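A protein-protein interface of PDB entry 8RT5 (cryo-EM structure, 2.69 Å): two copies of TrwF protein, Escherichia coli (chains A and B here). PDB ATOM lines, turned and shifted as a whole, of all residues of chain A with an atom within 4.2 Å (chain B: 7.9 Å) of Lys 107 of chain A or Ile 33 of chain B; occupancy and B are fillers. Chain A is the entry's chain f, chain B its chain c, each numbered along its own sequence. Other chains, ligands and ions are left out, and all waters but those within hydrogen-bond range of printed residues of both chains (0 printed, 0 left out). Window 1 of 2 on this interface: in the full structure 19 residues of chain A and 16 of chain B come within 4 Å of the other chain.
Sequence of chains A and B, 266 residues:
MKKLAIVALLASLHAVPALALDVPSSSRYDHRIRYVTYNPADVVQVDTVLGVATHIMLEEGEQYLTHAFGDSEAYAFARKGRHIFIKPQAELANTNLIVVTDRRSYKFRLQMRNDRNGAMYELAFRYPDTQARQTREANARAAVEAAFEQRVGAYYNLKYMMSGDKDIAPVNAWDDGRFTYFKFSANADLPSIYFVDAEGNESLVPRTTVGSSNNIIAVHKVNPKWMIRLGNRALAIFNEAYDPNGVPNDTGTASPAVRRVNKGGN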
ATOM      1  N   PRO A  40      -3.476   2.704  -2.076  1.00  0.00           N
ATOM      2  CA  PRO A  40      -3.757   2.791  -3.516  1.00  0.00           C
ATOM      3  C   PRO A  40      -5.120   2.256  -3.903  1.00  0.00           C
ATOM      4  O   PRO A  40      -5.622   2.613  -4.973  1.00  0.00           O
ATOM      5  CB  PRO A  40      -2.639   1.949  -4.144  1.00  0.00           C
ATOM      6  CG  PRO A  40      -1.595   1.856  -3.102  1.00  0.00           C
ATOM      7  CD  PRO A  40      -2.309   1.860  -1.799  1.00  0.00           C
ATOM      8  N   ALA A  41      -5.732   1.415  -3.078  1.00  0.00           N
ATOM      9  CA  ALA A  41      -6.998   0.777  -3.401  1.00  0.00           C
ATOM     10  C   ALA A  41      -8.166   1.391  -2.639  1.00  0.00           C
ATOM     11  O   ALA A  41      -9.186   0.734  -2.428  1.00  0.00           O
ATOM     12  CB  ALA A  41      -6.918  -0.722  -3.130  1.00  0.00           C
ATOM     13  N   ASP A  42      -8.042   2.652  -2.230  1.00  0.00           N
ATOM     14  CA  ASP A  42      -9.106   3.296  -1.477  1.00  0.00           C
ATOM     15  C   ASP A  42      -9.211   4.756  -1.886  1.00  0.00           C
ATOM     16  O   ASP A  42      -8.304   5.320  -2.501  1.00  0.00           O
ATOM     17  CB  ASP A  42      -8.882   3.180   0.032  1.00  0.00           C
ATOM     18  CG  ASP A  42     -10.168   3.291   0.817  1.00  0.00           C
ATOM     19  OD1 ASP A  42     -11.227   3.478   0.189  1.00  0.00           O
ATOM     20  OD2 ASP A  42     -10.126   3.184   2.059  1.00  0.00           O
ATOM     21  N   VAL A  43     -10.347   5.355  -1.547  1.00  0.00           N
ATOM     22  CA  VAL A  43     -10.637   6.746  -1.850  1.00  0.00           C
ATOM     23  C   VAL A  43     -10.687   7.522  -0.542  1.00  0.00           C
ATOM     24  O   VAL A  43     -11.172   7.037   0.484  1.00  0.00           O
ATOM     25  CB  VAL A  43     -11.957   6.890  -2.637  1.00  0.00           C
ATOM     26  CG1 VAL A  43     -12.266   8.341  -2.922  1.00  0.00           C
ATOM     27  CG2 VAL A  43     -11.893   6.110  -3.925  1.00  0.00           C
ATOM     28  N   VAL A  44     -10.184   8.752  -0.584  1.00  0.00           N
ATOM     29  CA  VAL A  44     -10.095   9.617   0.586  1.00  0.00           C
ATOM     30  C   VAL A  44     -11.284  10.561   0.575  1.00  0.00           C
ATOM     31  O   VAL A  44     -11.532  11.244  -0.423  1.00  0.00           O
ATOM     32  CB  VAL A  44      -8.771  10.401   0.611  1.00  0.00           C
ATOM     33  CG1 VAL A  44      -8.774  11.406   1.738  1.00  0.00           C
ATOM     34  CG2 VAL A  44      -7.599   9.460   0.745  1.00  0.00           C
ATOM     35  N   LEU A  97     -11.945  14.107  -7.257  1.00  0.00           N
ATOM     36  CA  LEU A  97     -10.669  14.621  -7.724  1.00  0.00           C
ATOM     37  C   LEU A  97      -9.669  13.480  -7.769  1.00  0.00           C
ATOM     38  O   LEU A  97      -9.568  12.703  -6.817  1.00  0.00           O
ATOM     39  CB  LEU A  97     -10.164  15.741  -6.815  1.00  0.00           C
ATOM     40  CG  LEU A  97      -8.761  16.290  -7.054  1.00  0.00           C
ATOM     41  CD1 LEU A  97      -8.637  16.896  -8.435  1.00  0.00           C
ATOM     42  CD2 LEU A  97      -8.421  17.303  -5.992  1.00  0.00           C
ATOM     43  N   SER A 105      -1.328   7.751  -7.581  1.00  0.00           N
ATOM     44  CA  SER A 105      -2.479   8.581  -7.907  1.00  0.00           C
ATOM     45  C   SER A 105      -3.378   8.665  -6.684  1.00  0.00           C
ATOM     46  O   SER A 105      -3.621   7.655  -6.019  1.00  0.00           O
ATOM     47  CB  SER A 105      -3.257   8.030  -9.101  1.00  0.00           C
ATOM     48  OG  SER A 105      -3.945   6.848  -8.762  1.00  0.00           O
ATOM     49  N   TYR A 106      -3.863   9.865  -6.388  1.00  0.00           N
ATOM     50  CA  TYR A 106      -4.706  10.115  -5.228  1.00  0.00           C
ATOM     51  C   TYR A 106      -6.159  10.220  -5.658  1.00  0.00           C
ATOM     52  O   TYR A 106      -6.466  10.863  -6.663  1.00  0.00           O
ATOM     53  CB  TYR A 106      -4.291  11.399  -4.516  1.00  0.00           C
ATOM     54  CG  TYR A 106      -2.858  11.443  -4.061  1.00  0.00           C
ATOM     55  CD1 TYR A 106      -2.517  11.118  -2.761  1.00  0.00           C
ATOM     56  CD2 TYR A 106      -1.850  11.819  -4.929  1.00  0.00           C
ATOM     57  CE1 TYR A 106      -1.217  11.166  -2.342  1.00  0.00           C
ATOM     58  CE2 TYR A 106      -0.551  11.865  -4.520  1.00  0.00           C
ATOM     59  CZ  TYR A 106      -0.236  11.541  -3.224  1.00  0.00           C
ATOM     60  OH  TYR A 106       1.069  11.588  -2.806  1.00  0.00           O
ATOM     61  N   LYS A 107      -7.048   9.598  -4.894  1.00  0.00           N
ATOM     62  CA  LYS A 107      -8.477   9.608  -5.174  1.00  0.00           C
ATOM     63  C   LYS A 107      -9.192  10.311  -4.032  1.00  0.00           C
ATOM     64  O   LYS A 107      -9.135   9.855  -2.888  1.00  0.00           O
ATOM     65  CB  LYS A 107      -9.015   8.187  -5.351  1.00  0.00           C
ATOM     66  CG  LYS A 107      -8.903   7.658  -6.761  1.00  0.00           C
ATOM     67  CD  LYS A 107      -7.495   7.211  -7.076  1.00  0.00           C
ATOM     68  CE  LYS A 107      -7.143   5.930  -6.359  1.00  0.00           C
ATOM     69  NZ  LYS A 107      -5.795   5.452  -6.732  1.00  0.00           N
ATOM     70  N   PHE A 108      -9.860  11.412  -4.347  1.00  0.00           N
ATOM     71  CA  PHE A 108     -10.589  12.202  -3.373  1.00  0.00           C
ATOM     72  C   PHE A 108     -12.057  12.271  -3.752  1.00  0.00           C
ATOM     73  O   PHE A 108     -12.402  12.514  -4.909  1.00  0.00           O
ATOM     74  CB  PHE A 108     -10.035  13.625  -3.287  1.00  0.00           C
ATOM     75  CG  PHE A 108      -8.575  13.690  -2.995  1.00  0.00           C
ATOM     76  CD1 PHE A 108      -8.104  13.470  -1.719  1.00  0.00           C
ATOM     77  CD2 PHE A 108      -7.674  13.991  -3.993  1.00  0.00           C
ATOM     78  CE1 PHE A 108      -6.768  13.537  -1.449  1.00  0.00           C
ATOM     79  CE2 PHE A 108      -6.336  14.060  -3.724  1.00  0.00           C
ATOM     80  CZ  PHE A 108      -5.882  13.831  -2.453  1.00  0.00           C
ATOM     81  N   PRO B  24     -15.791  -5.198 -14.373  1.00  0.00           N
ATOM     82  CA  PRO B  24     -14.647  -5.089 -13.466  1.00  0.00           C
ATOM     83  C   PRO B  24     -15.033  -5.380 -12.026  1.00  0.00           C
ATOM     84  O   PRO B  24     -16.175  -5.180 -11.610  1.00  0.00           O
ATOM     85  CB  PRO B  24     -14.198  -3.634 -13.638  1.00  0.00           C
ATOM     86  CG  PRO B  24     -14.738  -3.225 -14.945  1.00  0.00           C
ATOM     87  CD  PRO B  24     -16.039  -3.942 -15.089  1.00  0.00           C
ATOM     88  N   SER B  25     -14.059  -5.861 -11.264  1.00  0.00           N
ATOM     89  CA  SER B  25     -14.258  -6.230  -9.871  1.00  0.00           C
ATOM     90  C   SER B  25     -13.736  -5.124  -8.965  1.00  0.00           C
ATOM     91  O   SER B  25     -12.707  -4.508  -9.258  1.00  0.00           O
ATOM     92  CB  SER B  25     -13.557  -7.549  -9.554  1.00  0.00           C
ATOM     93  OG  SER B  25     -12.168  -7.352  -9.389  1.00  0.00           O
ATOM     94  N   SER B  26     -14.448  -4.877  -7.870  1.00  0.00           N
ATOM     95  CA  SER B  26     -14.090  -3.815  -6.945  1.00  0.00           C
ATOM     96  C   SER B  26     -12.992  -4.267  -5.986  1.00  0.00           C
ATOM     97  O   SER B  26     -12.736  -5.460  -5.807  1.00  0.00           O
ATOM     98  CB  SER B  26     -15.314  -3.370  -6.149  1.00  0.00           C
ATOM     99  OG  SER B  26     -16.397  -3.073  -7.007  1.00  0.00           O
ATOM    100  N   SER B  27     -12.336  -3.290  -5.365  1.00  0.00           N
ATOM    101  CA  SER B  27     -11.391  -3.596  -4.306  1.00  0.00           C
ATOM    102  C   SER B  27     -12.132  -3.830  -2.993  1.00  0.00           C
ATOM    103  O   SER B  27     -13.300  -3.471  -2.831  1.00  0.00           O
ATOM    104  CB  SER B  27     -10.373  -2.470  -4.140  1.00  0.00           C
ATOM    105  OG  SER B  27     -11.016  -1.228  -3.941  1.00  0.00           O
ATOM    106  N   ARG B  28     -11.436  -4.441  -2.041  1.00  0.00           N
ATOM    107  CA  ARG B  28     -12.035  -4.732  -0.748  1.00  0.00           C
ATOM    108  C   ARG B  28     -12.200  -3.496   0.122  1.00  0.00           C
ATOM    109  O   ARG B  28     -12.902  -3.562   1.136  1.00  0.00           O
ATOM    110  CB  ARG B  28     -11.199  -5.772  -0.004  1.00  0.00           C
ATOM    111  CG  ARG B  28      -9.824  -5.285   0.392  1.00  0.00           C
ATOM    112  CD  ARG B  28      -9.014  -6.401   1.014  1.00  0.00           C
ATOM    113  NE  ARG B  28      -7.713  -5.933   1.477  1.00  0.00           N
ATOM    114  CZ  ARG B  28      -6.628  -5.877   0.713  1.00  0.00           C
ATOM    115  NH1 ARG B  28      -6.687  -6.255  -0.555  1.00  0.00           N
ATOM    116  NH2 ARG B  28      -5.485  -5.439   1.218  1.00  0.00           N
ATOM    117  N   TYR B  29     -11.580  -2.377  -0.245  1.00  0.00           N
ATOM    118  CA  TYR B  29     -11.718  -1.157   0.541  1.00  0.00           C
ATOM    119  C   TYR B  29     -12.879  -0.306   0.048  1.00  0.00           C
ATOM    120  O   TYR B  29     -13.816  -0.020   0.799  1.00  0.00           O
ATOM    121  CB  TYR B  29     -10.414  -0.363   0.509  1.00  0.00           C
ATOM    122  CG  TYR B  29      -9.233  -1.133   1.036  1.00  0.00           C
ATOM    123  CD1 TYR B  29      -9.129  -1.437   2.385  1.00  0.00           C
ATOM    124  CD2 TYR B  29      -8.227  -1.563   0.189  1.00  0.00           C
ATOM    125  CE1 TYR B  29      -8.054  -2.139   2.876  1.00  0.00           C
ATOM    126  CE2 TYR B  29      -7.148  -2.266   0.669  1.00  0.00           C
ATOM    127  CZ  TYR B  29      -7.066  -2.551   2.012  1.00  0.00           C
ATOM    128  OH  TYR B  29      -5.988  -3.255   2.490  1.00  0.00           O
ATOM    129  N   ASP B  30     -12.839   0.106  -1.212  1.00  0.00           N
ATOM    130  CA  ASP B  30     -13.877   0.954  -1.771  1.00  0.00           C
ATOM    131  C   ASP B  30     -14.335   0.388  -3.105  1.00  0.00           C
ATOM    132  O   ASP B  30     -13.533  -0.160  -3.864  1.00  0.00           O
ATOM    133  CB  ASP B  30     -13.379   2.388  -1.959  1.00  0.00           C
ATOM    134  CG  ASP B  30     -14.510   3.373  -2.111  1.00  0.00           C
ATOM    135  OD1 ASP B  30     -15.112   3.422  -3.192  1.00  0.00           O
ATOM    136  OD2 ASP B  30     -14.804   4.097  -1.146  1.00  0.00           O
ATOM    137  N   HIS B  31     -15.627   0.530  -3.388  1.00  0.00           N
ATOM    138  CA  HIS B  31     -16.194   0.061  -4.645  1.00  0.00           C
ATOM    139  C   HIS B  31     -15.842   0.953  -5.829  1.00  0.00           C
ATOM    140  O   HIS B  31     -16.118   0.570  -6.968  1.00  0.00           O
ATOM    141  CB  HIS B  31     -17.716  -0.059  -4.519  1.00  0.00           C
ATOM    142  CG  HIS B  31     -18.414   1.251  -4.326  1.00  0.00           C
ATOM    143  ND1 HIS B  31     -18.617   2.145  -5.354  1.00  0.00           N
ATOM    144  CD2 HIS B  31     -18.939   1.826  -3.220  1.00  0.00           C
ATOM    145  CE1 HIS B  31     -19.247   3.210  -4.892  1.00  0.00           C
ATOM    146  NE2 HIS B  31     -19.452   3.042  -3.598  1.00  0.00           N
ATOM    147  N   ARG B  32     -15.253   2.121  -5.595  1.00  0.00           N
ATOM    148  CA  ARG B  32     -14.909   3.052  -6.659  1.00  0.00           C
ATOM    149  C   ARG B  32     -13.599   2.705  -7.347  1.00  0.00           C
ATOM    150  O   ARG B  32     -13.292   3.289  -8.390  1.00  0.00           O
ATOM    151  CB  ARG B  32     -14.833   4.473  -6.095  1.00  0.00           C
ATOM    152  CG  ARG B  32     -16.161   4.994  -5.592  1.00  0.00           C
ATOM    153  CD  ARG B  32     -16.011   6.301  -4.855  1.00  0.00           C
ATOM    154  NE  ARG B  32     -17.293   6.772  -4.341  1.00  0.00           N
ATOM    155  CZ  ARG B  32     -17.788   6.434  -3.157  1.00  0.00           C
ATOM    156  NH1 ARG B  32     -17.115   5.618  -2.362  1.00  0.00           N
ATOM    157  NH2 ARG B  32     -18.961   6.907  -2.769  1.00  0.00           N
ATOM    158  N   ILE B  33     -12.824   1.783  -6.789  1.00  0.00           N
ATOM    159  CA  ILE B  33     -11.586   1.306  -7.392  1.00  0.00           C
ATOM    160  C   ILE B  33     -11.850  -0.095  -7.920  1.00  0.00           C
ATOM    161  O   ILE B  33     -12.153  -1.009  -7.145  1.00  0.00           O
ATOM    162  CB  ILE B  33     -10.426   1.311  -6.385  1.00  0.00           C
ATOM    163  CG1 ILE B  33     -10.319   2.672  -5.696  1.00  0.00           C
ATOM    164  CG2 ILE B  33      -9.127   0.968  -7.074  1.00  0.00           C
ATOM    165  CD1 ILE B  33     -10.058   3.812  -6.642  1.00  0.00           C
ATOM    166  N   ARG B  34     -11.738  -0.268  -9.232  1.00  0.00           N
ATOM    167  CA  ARG B  34     -12.127  -1.513  -9.872  1.00  0.00           C
ATOM    168  C   ARG B  34     -11.005  -2.063 -10.739  1.00  0.00           C
ATOM    169  O   ARG B  34     -10.169  -1.323 -11.260  1.00  0.00           O
ATOM    170  CB  ARG B  34     -13.408  -1.337 -10.692  1.00  0.00           C
ATOM    171  CG  ARG B  34     -14.653  -1.450  -9.829  1.00  0.00           C
ATOM    172  CD  ARG B  34     -15.942  -1.405 -10.616  1.00  0.00           C
ATOM    173  NE  ARG B  34     -17.028  -0.860  -9.810  1.00  0.00           N
ATOM    174  CZ  ARG B  34     -17.852   0.104 -10.200  1.00  0.00           C
ATOM    175  NH1 ARG B  34     -17.741   0.630 -11.407  1.00  0.00           N
ATOM    176  NH2 ARG B  34     -18.803   0.530  -9.384  1.00  0.00           N
ATOM    177  N   TYR B  35     -10.994  -3.386 -10.862  1.00  0.00           N
ATOM    178  CA  TYR B  35      -9.956  -4.130 -11.559  1.00  0.00           C
ATOM    179  C   TYR B  35     -10.596  -5.038 -12.593  1.00  0.00           C
ATOM    180  O   TYR B  35     -11.689  -5.565 -12.376  1.00  0.00           O
ATOM    181  CB  TYR B  35      -9.143  -4.975 -10.583  1.00  0.00           C
ATOM    182  CG  TYR B  35      -8.588  -4.193  -9.426  1.00  0.00           C
ATOM    183  CD1 TYR B  35      -9.086  -4.371  -8.147  1.00  0.00           C
ATOM    184  CD2 TYR B  35      -7.545  -3.299  -9.605  1.00  0.00           C
ATOM    185  CE1 TYR B  35      -8.582  -3.661  -7.087  1.00  0.00           C
ATOM    186  CE2 TYR B  35      -7.033  -2.589  -8.550  1.00  0.00           C
ATOM    187  CZ  TYR B  35      -7.553  -2.774  -7.294  1.00  0.00           C
ATOM    188  OH  TYR B  35      -7.039  -2.065  -6.235  1.00  0.00           O
ATOM    189  N   ALA B  53     -15.219  11.744 -12.785  1.00  0.00           N
ATOM    190  CA  ALA B  53     -14.170  11.427 -13.736  1.00  0.00           C
ATOM    191  C   ALA B  53     -13.640  10.038 -13.424  1.00  0.00           C
ATOM    192  O   ALA B  53     -13.448   9.691 -12.257  1.00  0.00           O
ATOM    193  CB  ALA B  53     -13.042  12.455 -13.675  1.00  0.00           C
ATOM    194  N   HIS B  55     -10.535   7.369 -14.040  1.00  0.00           N
ATOM    195  CA  HIS B  55      -9.130   7.268 -14.404  1.00  0.00           C
ATOM    196  C   HIS B  55      -8.854   5.858 -14.908  1.00  0.00           C
ATOM    197  O   HIS B  55      -8.871   4.902 -14.133  1.00  0.00           O
ATOM    198  CB  HIS B  55      -8.247   7.607 -13.205  1.00  0.00           C
ATOM    199  CG  HIS B  55      -6.786   7.410 -13.452  1.00  0.00           C
ATOM    200  ND1 HIS B  55      -5.969   6.750 -12.562  1.00  0.00           N
ATOM    201  CD2 HIS B  55      -5.992   7.796 -14.476  1.00  0.00           C
ATOM    202  CE1 HIS B  55      -4.738   6.724 -13.034  1.00  0.00           C
ATOM    203  NE2 HIS B  55      -4.724   7.355 -14.194  1.00  0.00           N
ATOM    204  N   ALA B 119     -20.219   4.609  -8.530  1.00  0.00           N
ATOM    205  CA  ALA B 119     -19.288   5.242  -9.446  1.00  0.00           C
ATOM    206  C   ALA B 119     -17.989   4.449  -9.531  1.00  0.00           C
ATOM    207  O   ALA B 119     -17.654   3.646  -8.658  1.00  0.00           O
ATOM    208  CB  ALA B 119     -18.996   6.673  -9.006  1.00  0.00           C
ATOM    209  N   MET B 120     -17.254   4.683 -10.612  1.00  0.00           N
ATOM    210  CA  MET B 120     -15.936   4.100 -10.824  1.00  0.00           C
ATOM    211  C   MET B 120     -14.932   5.241 -10.911  1.00  0.00           C
ATOM    212  O   MET B 120     -15.033   6.094 -11.796  1.00  0.00           O
ATOM    213  CB  MET B 120     -15.909   3.246 -12.089  1.00  0.00           C
ATOM    214  CG  MET B 120     -14.650   2.411 -12.245  1.00  0.00           C
ATOM    215  SD  MET B 120     -14.424   1.758 -13.905  1.00  0.00           S
ATOM    216  CE  MET B 120     -15.930   0.815 -14.106  1.00  0.00           C
ATOM    217  N   TYR B 121     -13.969   5.261  -9.994  1.00  0.00           N
ATOM    218  CA  TYR B 121     -12.947   6.296 -10.007  1.00  0.00           C
ATOM    219  C   TYR B 121     -11.718   5.895 -10.805  1.00  0.00           C
ATOM    220  O   TYR B 121     -11.224   6.702 -11.597  1.00  0.00           O
ATOM    221  CB  TYR B 121     -12.526   6.653  -8.579  1.00  0.00           C
ATOM    222  CG  TYR B 121     -13.481   7.566  -7.848  1.00  0.00           C
ATOM    223  CD1 TYR B 121     -14.825   7.605  -8.175  1.00  0.00           C
ATOM    224  CD2 TYR B 121     -13.038   8.370  -6.813  1.00  0.00           C
ATOM    225  CE1 TYR B 121     -15.695   8.422  -7.509  1.00  0.00           C
ATOM    226  CE2 TYR B 121     -13.905   9.191  -6.133  1.00  0.00           C
ATOM    227  CZ  TYR B 121     -15.233   9.214  -6.486  1.00  0.00           C
ATOM    228  OH  TYR B 121     -16.104  10.035  -5.815  1.00  0.00           O
ATOM    229  N   GLU B 122     -11.213   4.678 -10.620  1.00  0.00           N
ATOM    230  CA  GLU B 122     -10.152   4.166 -11.473  1.00  0.00           C
ATOM    231  C   GLU B 122     -10.495   2.774 -11.964  1.00  0.00           C
ATOM    232  O   GLU B 122     -11.144   1.998 -11.259  1.00  0.00           O
ATOM    233  CB  GLU B 122      -8.783   4.118 -10.786  1.00  0.00           C
ATOM    234  CG  GLU B 122      -8.170   5.444 -10.459  1.00  0.00           C
ATOM    235  CD  GLU B 122      -6.829   5.286  -9.785  1.00  0.00           C
ATOM    236  OE1 GLU B 122      -6.461   4.138  -9.470  1.00  0.00           O
ATOM    237  OE2 GLU B 122      -6.123   6.298  -9.613  1.00  0.00           O
ATOM    238  N   LEU B 123     -10.042   2.475 -13.175  1.00  0.00           N
ATOM    239  CA  LEU B 123     -10.042   1.140 -13.741  1.00  0.00           C
ATOM    240  C   LEU B 123      -8.602   0.727 -13.996  1.00  0.00           C
ATOM    241  O   LEU B 123      -7.877   1.413 -14.721  1.00  0.00           O
ATOM    242  CB  LEU B 123     -10.844   1.106 -15.039  1.00  0.00           C
ATOM    243  CG  LEU B 123     -11.074  -0.265 -15.662  1.00  0.00           C
ATOM    244  CD1 LEU B 123     -11.629  -1.225 -14.634  1.00  0.00           C
ATOM    245  CD2 LEU B 123     -12.006  -0.137 -16.842  1.00  0.00           C
ATOM    246  N   ALA B 124      -8.189  -0.387 -13.406  1.00  0.00           N
ATOM    247  CA  ALA B 124      -6.840  -0.897 -13.585  1.00  0.00           C
ATOM    248  C   ALA B 124      -6.901  -2.245 -14.282  1.00  0.00           C
ATOM    249  O   ALA B 124      -7.771  -3.066 -13.986  1.00  0.00           O
ATOM    250  CB  ALA B 124      -6.112  -1.024 -12.248  1.00  0.00           C
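Lys 107 of chain A touches two residues of chain B. Printed residues of chain A within 4 Å of Ile 33 of chain B: Ala 41 and Lys 107. Printed residues of chain B within 4 Å of Ser 105 of chain A: Glu 122. Of the printed residues of chain B, Val 43 of chain A touches Tyr 121. Of the printed residues of chain B, Asp 42 of chain A touches Tyr 29 (3.7 Å) and Asp 30 (3.2 Å). Leu 123 of chain B touches none of the printed residues of chain A. Pro 40 of chain A touches none of the printed residues of chain B. The nearest residue of chain B that does not touch Lys 107 of chain A is Tyr 121 of chain B (4.2 Å). The nearest printed residue of chain A that does not touch Ile 33 of chain B is Val 43 of chain A (4.004 Å). The nearest printed residue of chain B that does not touch Ala 41 of chain A is Arg 28 of chain B (5.7 Å).
No position is printed for both chains. Of the 12 pairs that touch across the chains among the printed residues, none has its exchanged pair printed and touching as well.
The side-chain carboxylate (OE2) of Glu 122 of chain B sits at hydrogen-bond distance from the side-chain hydroxyl (OG) of Ser 105 of chain A, at 2.4 Å. O of Ala 41 of chain A lies within hydrogen-bond range of OG of Ser 27 of chain B. OE2 of Glu 122 of chain B is in salt-bridge range of NZ of Lys 107 of chain A.
Printed residues of chain A that touch a printed residue of chain B: Ala 41, Asp 42, Val 43, Ser 105, Lys 107 and Phe 108. Of the 20 printed residues of chain B, 7 touch a printed residue of chain A. Hydrophobic or aromatic side chains of chain B within 4 Å of the printed part of chain A: Tyr 29, Ile 33, Tyr 35 and Tyr 121.
O of Arg 32 of chain B is in hydrogen-bond range of N of Tyr 121 of chain B, at 2.6 Å. The backbone carbonyl oxygen (O) of Leu 97 of chain A lies within hydrogen-bond range of the backbone NH (N) of Phe 108 of chain A, at 2.8 Å. The backbone NH (N) of Glu 122 of chain B sits at hydrogen-bond distance from the backbone carbonyl oxygen (O) of Arg 32 of chain B. The backbone carbonyl oxygen (O) of Asp 30 of chain B sits at hydrogen-bond distance from the side-chain hydroxyl (OG) of Ser 27 of chain B (2.7 Å). NZ of Lys 107 of chain A lies within hydrogen-bond range of O of Pro 40 of chain A (3.3 Å). NZ of Lys 107 of chain A lies within hydrogen-bond range of OG of Ser 105 of chain A (3.1 Å).
Among the printed residues, merely in contact across the chains: Ala 41 of chain A with Tyr 29 of chain B (3.4 Å), Ala 41 of chain A with Asp 30 of chain B (3.9 Å), Ala 41 of chain A with Ile 33 of chain B (3.95 Å), Ala 41 of chain A with Tyr 35 of chain B (3.4 Å), Asp 42 of chain A with Tyr 29 of chain B (3.7 Å), Asp 42 of chain A with Asp 30 of chain B (3.2 Å), Val 43 of chain A with Tyr 121 of chain B (3.7 Å), Lys 107 of chain A with Ile 33 of chain B (3.6 Å) and Phe 108 of chain A with Tyr 121 of chain B (3.8 Å).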
